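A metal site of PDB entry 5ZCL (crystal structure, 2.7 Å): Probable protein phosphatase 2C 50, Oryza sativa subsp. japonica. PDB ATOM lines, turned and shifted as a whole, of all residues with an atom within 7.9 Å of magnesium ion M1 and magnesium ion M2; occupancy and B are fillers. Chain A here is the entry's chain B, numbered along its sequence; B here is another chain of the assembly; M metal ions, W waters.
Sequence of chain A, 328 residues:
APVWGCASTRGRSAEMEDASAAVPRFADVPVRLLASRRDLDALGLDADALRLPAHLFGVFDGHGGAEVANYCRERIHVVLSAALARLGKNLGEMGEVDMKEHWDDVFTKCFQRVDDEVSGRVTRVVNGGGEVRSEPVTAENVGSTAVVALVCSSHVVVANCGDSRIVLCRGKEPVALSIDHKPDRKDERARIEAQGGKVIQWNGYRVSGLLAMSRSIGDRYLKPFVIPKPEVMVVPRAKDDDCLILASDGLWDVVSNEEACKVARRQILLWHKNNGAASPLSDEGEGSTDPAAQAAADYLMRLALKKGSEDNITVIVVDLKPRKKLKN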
ATOM      1  N   SER A  13      -4.919 -13.180  11.778  1.00  0.00           N
ATOM      2  CA  SER A  13      -4.643 -14.488  11.198  1.00  0.00           C
ATOM      3  C   SER A  13      -5.672 -14.831  10.132  1.00  0.00           C
ATOM      4  O   SER A  13      -6.790 -14.306  10.099  1.00  0.00           O
ATOM      5  CB  SER A  13      -4.634 -15.586  12.261  1.00  0.00           C
ATOM      6  OG  SER A  13      -3.479 -15.504  13.079  1.00  0.00           O
ATOM      7  N   GLU A  15      -7.377 -17.624   9.501  1.00  0.00           N
ATOM      8  CA  GLU A  15      -8.560 -18.369   9.913  1.00  0.00           C
ATOM      9  C   GLU A  15      -8.697 -18.383  11.432  1.00  0.00           C
ATOM     10  O   GLU A  15      -7.742 -18.131  12.174  1.00  0.00           O
ATOM     11  CB  GLU A  15      -8.560 -19.789   9.348  1.00  0.00           C
ATOM     12  CG  GLU A  15      -8.929 -19.829   7.873  1.00  0.00           C
ATOM     13  CD  GLU A  15      -8.423 -21.078   7.180  1.00  0.00           C
ATOM     14  OE1 GLU A  15      -7.238 -21.411   7.360  1.00  0.00           O
ATOM     15  OE2 GLU A  15      -9.224 -21.725   6.470  1.00  0.00           O
ATOM     16  N   MET A  16      -9.913 -18.718  11.882  1.00  0.00           N
ATOM     17  CA  MET A  16     -10.221 -18.801  13.301  1.00  0.00           C
ATOM     18  C   MET A  16     -10.153 -20.252  13.751  1.00  0.00           C
ATOM     19  O   MET A  16     -10.870 -21.108  13.224  1.00  0.00           O
ATOM     20  CB  MET A  16     -11.604 -18.217  13.578  1.00  0.00           C
ATOM     21  CG  MET A  16     -11.999 -18.232  15.049  1.00  0.00           C
ATOM     22  SD  MET A  16     -10.733 -17.455  16.103  1.00  0.00           S
ATOM     23  CE  MET A  16     -11.743 -16.840  17.436  1.00  0.00           C
ATOM     24  N   GLU A  17      -9.273 -20.530  14.702  1.00  0.00           N
ATOM     25  CA  GLU A  17      -9.145 -21.853  15.284  1.00  0.00           C
ATOM     26  C   GLU A  17      -9.260 -21.868  16.801  1.00  0.00           C
ATOM     27  O   GLU A  17      -9.184 -22.945  17.401  1.00  0.00           O
ATOM     28  CB  GLU A  17      -7.821 -22.492  14.859  1.00  0.00           C
ATOM     29  CG  GLU A  17      -7.731 -22.713  13.365  1.00  0.00           C
ATOM     30  CD  GLU A  17      -6.363 -23.214  12.923  1.00  0.00           C
ATOM     31  OE1 GLU A  17      -5.377 -23.040  13.688  1.00  0.00           O
ATOM     32  OE2 GLU A  17      -6.277 -23.756  11.800  1.00  0.00           O
ATOM     33  N   ASP A  18      -9.437 -20.709  17.444  1.00  0.00           N
ATOM     34  CA  ASP A  18      -9.773 -20.669  18.854  1.00  0.00           C
ATOM     35  C   ASP A  18     -11.247 -20.997  19.038  1.00  0.00           C
ATOM     36  O   ASP A  18     -12.066 -20.722  18.158  1.00  0.00           O
ATOM     37  CB  ASP A  18      -9.490 -19.297  19.474  1.00  0.00           C
ATOM     38  CG  ASP A  18      -8.050 -19.142  19.990  1.00  0.00           C
ATOM     39  OD1 ASP A  18      -7.176 -19.982  19.676  1.00  0.00           O
ATOM     40  OD2 ASP A  18      -7.813 -18.167  20.736  1.00  0.00           O
ATOM     41  N   PHE A  60     -10.028 -23.174  24.094  1.00  0.00           N
ATOM     42  CA  PHE A  60      -9.447 -24.254  23.289  1.00  0.00           C
ATOM     43  C   PHE A  60      -8.778 -23.650  22.055  1.00  0.00           C
ATOM     44  O   PHE A  60      -9.469 -23.262  21.105  1.00  0.00           O
ATOM     45  CB  PHE A  60     -10.516 -25.258  22.886  1.00  0.00           C
ATOM     46  CG  PHE A  60     -11.477 -25.565  23.976  1.00  0.00           C
ATOM     47  CD1 PHE A  60     -11.199 -26.549  24.906  1.00  0.00           C
ATOM     48  CD2 PHE A  60     -12.656 -24.845  24.091  1.00  0.00           C
ATOM     49  CE1 PHE A  60     -12.099 -26.829  25.922  1.00  0.00           C
ATOM     50  CE2 PHE A  60     -13.561 -25.112  25.105  1.00  0.00           C
ATOM     51  CZ  PHE A  60     -13.289 -26.099  26.019  1.00  0.00           C
ATOM     52  N   ASP A  61      -7.458 -23.578  22.085  1.00  0.00           N
ATOM     53  CA  ASP A  61      -6.671 -23.099  20.944  1.00  0.00           C
ATOM     54  C   ASP A  61      -6.418 -24.277  20.015  1.00  0.00           C
ATOM     55  O   ASP A  61      -5.613 -25.174  20.332  1.00  0.00           O
ATOM     56  CB  ASP A  61      -5.369 -22.463  21.423  1.00  0.00           C
ATOM     57  CG  ASP A  61      -4.575 -21.817  20.294  1.00  0.00           C
ATOM     58  OD1 ASP A  61      -4.763 -22.210  19.122  1.00  0.00           O
ATOM     59  OD2 ASP A  61      -3.764 -20.909  20.594  1.00  0.00           O
ATOM     60  N   GLY A  62      -7.097 -24.298  18.870  1.00  0.00           N
ATOM     61  CA  GLY A  62      -6.862 -25.323  17.888  1.00  0.00           C
ATOM     62  C   GLY A  62      -5.613 -25.081  17.065  1.00  0.00           C
ATOM     63  O   GLY A  62      -5.144 -23.950  16.907  1.00  0.00           O
ATOM     64  N   HIS A  63      -5.036 -26.171  16.557  1.00  0.00           N
ATOM     65  CA  HIS A  63      -3.976 -26.099  15.561  1.00  0.00           C
ATOM     66  C   HIS A  63      -4.239 -27.138  14.472  1.00  0.00           C
ATOM     67  O   HIS A  63      -4.838 -28.195  14.729  1.00  0.00           O
ATOM     68  CB  HIS A  63      -2.593 -26.330  16.185  1.00  0.00           C
ATOM     69  CG  HIS A  63      -2.518 -27.510  17.105  1.00  0.00           C
ATOM     70  ND1 HIS A  63      -2.449 -27.372  18.477  1.00  0.00           N
ATOM     71  CD2 HIS A  63      -2.506 -28.844  16.866  1.00  0.00           C
ATOM     72  CE1 HIS A  63      -2.390 -28.569  19.040  1.00  0.00           C
ATOM     73  NE2 HIS A  63      -2.432 -29.477  18.074  1.00  0.00           N
ATOM     74  N   GLY A  64      -3.800 -26.825  13.254  1.00  0.00           N
ATOM     75  CA  GLY A  64      -4.079 -27.688  12.120  1.00  0.00           C
ATOM     76  C   GLY A  64      -5.529 -27.721  11.670  1.00  0.00           C
ATOM     77  O   GLY A  64      -5.877 -28.492  10.779  1.00  0.00           O
ATOM     78  N   GLY A  65      -6.379 -26.892  12.250  1.00  0.00           N
ATOM     79  CA  GLY A  65      -7.797 -26.899  11.966  1.00  0.00           C
ATOM     80  C   GLY A  65      -8.578 -26.455  13.188  1.00  0.00           C
ATOM     81  O   GLY A  65      -8.049 -26.344  14.290  1.00  0.00           O
ATOM     82  N   ALA A  69     -10.918 -27.988  18.483  1.00  0.00           N
ATOM     83  CA  ALA A  69     -11.282 -26.945  19.436  1.00  0.00           C
ATOM     84  C   ALA A  69     -12.799 -26.814  19.517  1.00  0.00           C
ATOM     85  O   ALA A  69     -13.374 -26.728  20.613  1.00  0.00           O
ATOM     86  CB  ALA A  69     -10.640 -25.613  19.056  1.00  0.00           C
ATOM     87  N   GLY A 143      -5.542 -30.795  16.321  1.00  0.00           N
ATOM     88  CA  GLY A 143      -5.640 -30.886  17.771  1.00  0.00           C
ATOM     89  C   GLY A 143      -6.084 -29.587  18.396  1.00  0.00           C
ATOM     90  O   GLY A 143      -6.501 -28.653  17.698  1.00  0.00           O
ATOM     91  N   SER A 144      -5.999 -29.501  19.721  1.00  0.00           N
ATOM     92  CA  SER A 144      -6.387 -28.270  20.389  1.00  0.00           C
ATOM     93  C   SER A 144      -5.877 -28.267  21.809  1.00  0.00           C
ATOM     94  O   SER A 144      -5.805 -29.320  22.443  1.00  0.00           O
ATOM     95  CB  SER A 144      -7.909 -28.080  20.402  1.00  0.00           C
ATOM     96  OG  SER A 144      -8.233 -26.953  21.188  1.00  0.00           O
ATOM     97  N   THR A 145      -5.464 -27.101  22.283  1.00  0.00           N
ATOM     98  CA  THR A 145      -5.275 -26.942  23.715  1.00  0.00           C
ATOM     99  C   THR A 145      -6.633 -27.000  24.415  1.00  0.00           C
ATOM    100  O   THR A 145      -7.685 -26.831  23.792  1.00  0.00           O
ATOM    101  CB  THR A 145      -4.584 -25.616  24.041  1.00  0.00           C
ATOM    102  OG1 THR A 145      -5.435 -24.521  23.687  1.00  0.00           O
ATOM    103  CG2 THR A 145      -3.265 -25.515  23.303  1.00  0.00           C
ATOM    104  N   ASP A 163      -0.696 -25.060  25.820  1.00  0.00           N
ATOM    105  CA  ASP A 163      -0.022 -23.807  26.137  1.00  0.00           C
ATOM    106  C   ASP A 163      -0.995 -22.645  26.325  1.00  0.00           C
ATOM    107  O   ASP A 163      -0.547 -21.486  26.380  1.00  0.00           O
ATOM    108  CB  ASP A 163       1.044 -23.456  25.090  1.00  0.00           C
ATOM    109  CG  ASP A 163       0.480 -23.260  23.674  1.00  0.00           C
ATOM    110  OD1 ASP A 163      -0.707 -22.902  23.515  1.00  0.00           O
ATOM    111  OD2 ASP A 163       1.254 -23.450  22.711  1.00  0.00           O
ATOM    112  N   SER A 164      -2.298 -22.909  26.407  1.00  0.00           N
ATOM    113  CA  SER A 164      -3.214 -21.912  26.938  1.00  0.00           C
ATOM    114  C   SER A 164      -2.994 -21.766  28.451  1.00  0.00           C
ATOM    115  O   SER A 164      -2.287 -22.559  29.076  1.00  0.00           O
ATOM    116  CB  SER A 164      -4.657 -22.292  26.638  1.00  0.00           C
ATOM    117  OG  SER A 164      -4.933 -22.182  25.258  1.00  0.00           O
ATOM    118  N   MET A 213       3.933 -27.924  21.812  1.00  0.00           N
ATOM    119  CA  MET A 213       3.428 -28.263  23.132  1.00  0.00           C
ATOM    120  C   MET A 213       3.502 -29.777  23.288  1.00  0.00           C
ATOM    121  O   MET A 213       3.550 -30.518  22.300  1.00  0.00           O
ATOM    122  CB  MET A 213       1.990 -27.768  23.349  1.00  0.00           C
ATOM    123  CG  MET A 213       0.931 -28.461  22.511  1.00  0.00           C
ATOM    124  SD  MET A 213      -0.595 -27.496  22.413  1.00  0.00           S
ATOM    125  CE  MET A 213       0.025 -25.952  21.754  1.00  0.00           C
ATOM    126  N   SER A 248      -6.092 -17.938  25.436  1.00  0.00           N
ATOM    127  CA  SER A 248      -5.170 -18.639  24.563  1.00  0.00           C
ATOM    128  C   SER A 248      -3.854 -17.876  24.462  1.00  0.00           C
ATOM    129  O   SER A 248      -3.742 -16.723  24.907  1.00  0.00           O
ATOM    130  CB  SER A 248      -5.796 -18.837  23.182  1.00  0.00           C
ATOM    131  OG  SER A 248      -6.218 -17.599  22.655  1.00  0.00           O
ATOM    132  N   ASP A 249      -2.836 -18.521  23.870  1.00  0.00           N
ATOM    133  CA  ASP A 249      -1.547 -17.856  23.686  1.00  0.00           C
ATOM    134  C   ASP A 249      -1.681 -16.519  22.958  1.00  0.00           C
ATOM    135  O   ASP A 249      -0.832 -15.643  23.122  1.00  0.00           O
ATOM    136  CB  ASP A 249      -0.542 -18.764  22.947  1.00  0.00           C
ATOM    137  CG  ASP A 249      -1.064 -19.275  21.605  1.00  0.00           C
ATOM    138  OD1 ASP A 249      -2.177 -18.900  21.165  1.00  0.00           O
ATOM    139  OD2 ASP A 249      -0.327 -20.048  20.963  1.00  0.00           O
ATOM    140  N   GLY A 250      -2.749 -16.334  22.179  1.00  0.00           N
ATOM    141  CA  GLY A 250      -2.994 -15.079  21.494  1.00  0.00           C
ATOM    142  C   GLY A 250      -2.965 -13.862  22.397  1.00  0.00           C
ATOM    143  O   GLY A 250      -2.805 -12.737  21.927  1.00  0.00           O
ATOM    144  N   LEU A 251      -3.165 -14.072  23.699  1.00  0.00           N
ATOM    145  CA  LEU A 251      -3.060 -13.016  24.696  1.00  0.00           C
ATOM    146  C   LEU A 251      -1.780 -13.101  25.532  1.00  0.00           C
ATOM    147  O   LEU A 251      -1.165 -12.064  25.800  1.00  0.00           O
ATOM    148  CB  LEU A 251      -4.274 -13.037  25.628  1.00  0.00           C
ATOM    149  CG  LEU A 251      -4.212 -12.052  26.791  1.00  0.00           C
ATOM    150  CD1 LEU A 251      -4.849 -10.709  26.410  1.00  0.00           C
ATOM    151  CD2 LEU A 251      -4.861 -12.627  28.037  1.00  0.00           C
ATOM    152  N   ASP A 253       1.131 -14.390  24.825  1.00  0.00           N
ATOM    153  CA  ASP A 253       2.370 -14.172  24.087  1.00  0.00           C
ATOM    154  C   ASP A 253       2.795 -12.700  24.069  1.00  0.00           C
ATOM    155  O   ASP A 253       3.977 -12.423  23.824  1.00  0.00           O
ATOM    156  CB  ASP A 253       2.234 -14.693  22.655  1.00  0.00           C
ATOM    157  CG  ASP A 253       2.428 -16.204  22.541  1.00  0.00           C
ATOM    158  OD1 ASP A 253       3.183 -16.771  23.358  1.00  0.00           O
ATOM    159  OD2 ASP A 253       1.831 -16.823  21.627  1.00  0.00           O
ATOM    160  N   ASP A 311      -1.793 -13.850  16.274  1.00  0.00           N
ATOM    161  CA  ASP A 311      -2.559 -15.079  16.421  1.00  0.00           C
ATOM    162  C   ASP A 311      -4.001 -14.764  16.787  1.00  0.00           C
ATOM    163  O   ASP A 311      -4.346 -13.625  17.134  1.00  0.00           O
ATOM    164  CB  ASP A 311      -1.914 -15.966  17.499  1.00  0.00           C
ATOM    165  CG  ASP A 311      -2.574 -17.331  17.601  1.00  0.00           C
ATOM    166  OD1 ASP A 311      -3.284 -17.736  16.642  1.00  0.00           O
ATOM    167  OD2 ASP A 311      -2.372 -18.009  18.628  1.00  0.00           O
ATOM    168  N   ASN A 312      -4.860 -15.772  16.669  1.00  0.00           N
ATOM    169  CA  ASN A 312      -6.188 -15.689  17.262  1.00  0.00           C
ATOM    170  C   ASN A 312      -6.053 -15.334  18.750  1.00  0.00           C
ATOM    171  O   ASN A 312      -5.059 -15.673  19.402  1.00  0.00           O
ATOM    172  CB  ASN A 312      -6.943 -17.009  17.132  1.00  0.00           C
ATOM    173  CG  ASN A 312      -7.095 -17.482  15.702  1.00  0.00           C
ATOM    174  OD1 ASN A 312      -7.166 -18.680  15.441  1.00  0.00           O
ATOM    175  ND2 ASN A 312      -7.145 -16.540  14.773  1.00  0.00           N
ATOM    176  N   ILE A 313      -7.076 -14.667  19.283  1.00  0.00           N
ATOM    177  CA  ILE A 313      -7.084 -14.238  20.672  1.00  0.00           C
ATOM    178  C   ILE A 313      -8.443 -14.528  21.277  1.00  0.00           C
ATOM    179  O   ILE A 313      -9.470 -14.091  20.738  1.00  0.00           O
ATOM    180  CB  ILE A 313      -6.733 -12.749  20.833  1.00  0.00           C
ATOM    181  CG1 ILE A 313      -5.292 -12.492  20.405  1.00  0.00           C
ATOM    182  CG2 ILE A 313      -6.947 -12.306  22.264  1.00  0.00           C
ATOM    183  CD1 ILE A 313      -4.927 -11.029  20.331  1.00  0.00           C
ATOM    184  N   SER B  71      -1.544 -24.239  10.449  1.00  0.00           N
ATOM    185  CA  SER B  71      -0.967 -23.772  11.696  1.00  0.00           C
ATOM    186  C   SER B  71      -0.453 -24.937  12.544  1.00  0.00           C
ATOM    187  O   SER B  71      -0.760 -26.109  12.297  1.00  0.00           O
ATOM    188  CB  SER B  71      -2.002 -22.972  12.490  1.00  0.00           C
ATOM    189  OG  SER B  71      -3.145 -23.771  12.745  1.00  0.00           O
ATOM    190  N   GLY B  72       0.329 -24.593  13.564  1.00  0.00           N
ATOM    191  CA  GLY B  72       0.933 -25.586  14.434  1.00  0.00           C
ATOM    192  C   GLY B  72       2.200 -26.203  13.887  1.00  0.00           C
ATOM    193  O   GLY B  72       2.549 -27.328  14.279  1.00  0.00           O
HETATM  194 MG    MG M   1      -2.303 -20.015  19.167  1.00  0.00          MG
HETATM  195 MG    MG M   2      -4.111 -21.692  17.271  1.00  0.00          MG
HETATM  196  O   HOH W   1      -2.129 -22.902  17.310  1.00  0.00           O
HETATM  197  O   HOH W   2      -4.311 -18.690  20.010  1.00  0.00           O
HETATM  198  O   HOH W   3      -5.596 -20.400  17.346  1.00  0.00           O
HETATM  199  O   HOH W   4      -3.955 -21.717  15.359  1.00  0.00           O
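The backbone NH (N) of Thr 145 is in hydrogen-bond range of the backbone carbonyl oxygen (O) of Asp 61 (2.7 Å).
O of Asp 61 lies close to OG of Ser 144.
O of Glu 17 sits at hydrogen-bond distance from N of Gly 62, 2.9 Å away.
Within 4 Å of magnesium ion M2: Asp 61 and Gly 62.
The nearest printed residue that does not touch magnesium ion M2 is Glu 17 (4.03 Å).
Magnesium ion M1 is bound by OD2 of Asp 311 (2.1 Å).
Magnesium ion M1 is bound by OD2 of Asp 61 (2.2 Å).
Magnesium ion M1 is bound by OD1 of Asp 249 (2.3 Å).
Magnesium ion M1 is bound by water W2, at 2.5 Å.
Magnesium ion M1 has four donor atoms within binding distance.
Slightly farther from magnesium ion M1 lies the side-chain carboxylate (OD2) of Asp 249 (2.7 Å).
Water W4 is bound to magnesium ion M2 (1.9 Å).
Water W3 is bound to magnesium ion M2, at 2.0 Å.
Magnesium ion M2 is bound by OD1 of Asp 61 (2.0 Å).
Water W1 binds magnesium ion M2 (2.3 Å).
The backbone carbonyl oxygen (O) of Gly 62 is bound to magnesium ion M2, 2.5 Å away.
Water W2 lies within hydrogen-bond range of the side-chain carboxylate of Asp 18 (3.2 Å), the backbone carbonyl oxygen of Asn 312 (3.2 Å) and the side-chain hydroxyl of Ser 248 (3.4 Å).
Water W3 lies within hydrogen-bond range of OD1 of Asp 18 (2.8 Å) and OD1 of Asn 312 (3.0 Å).
Water W4 lies within hydrogen-bond range of OE1 of Glu 17 and OG of Ser 71 of chain B.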
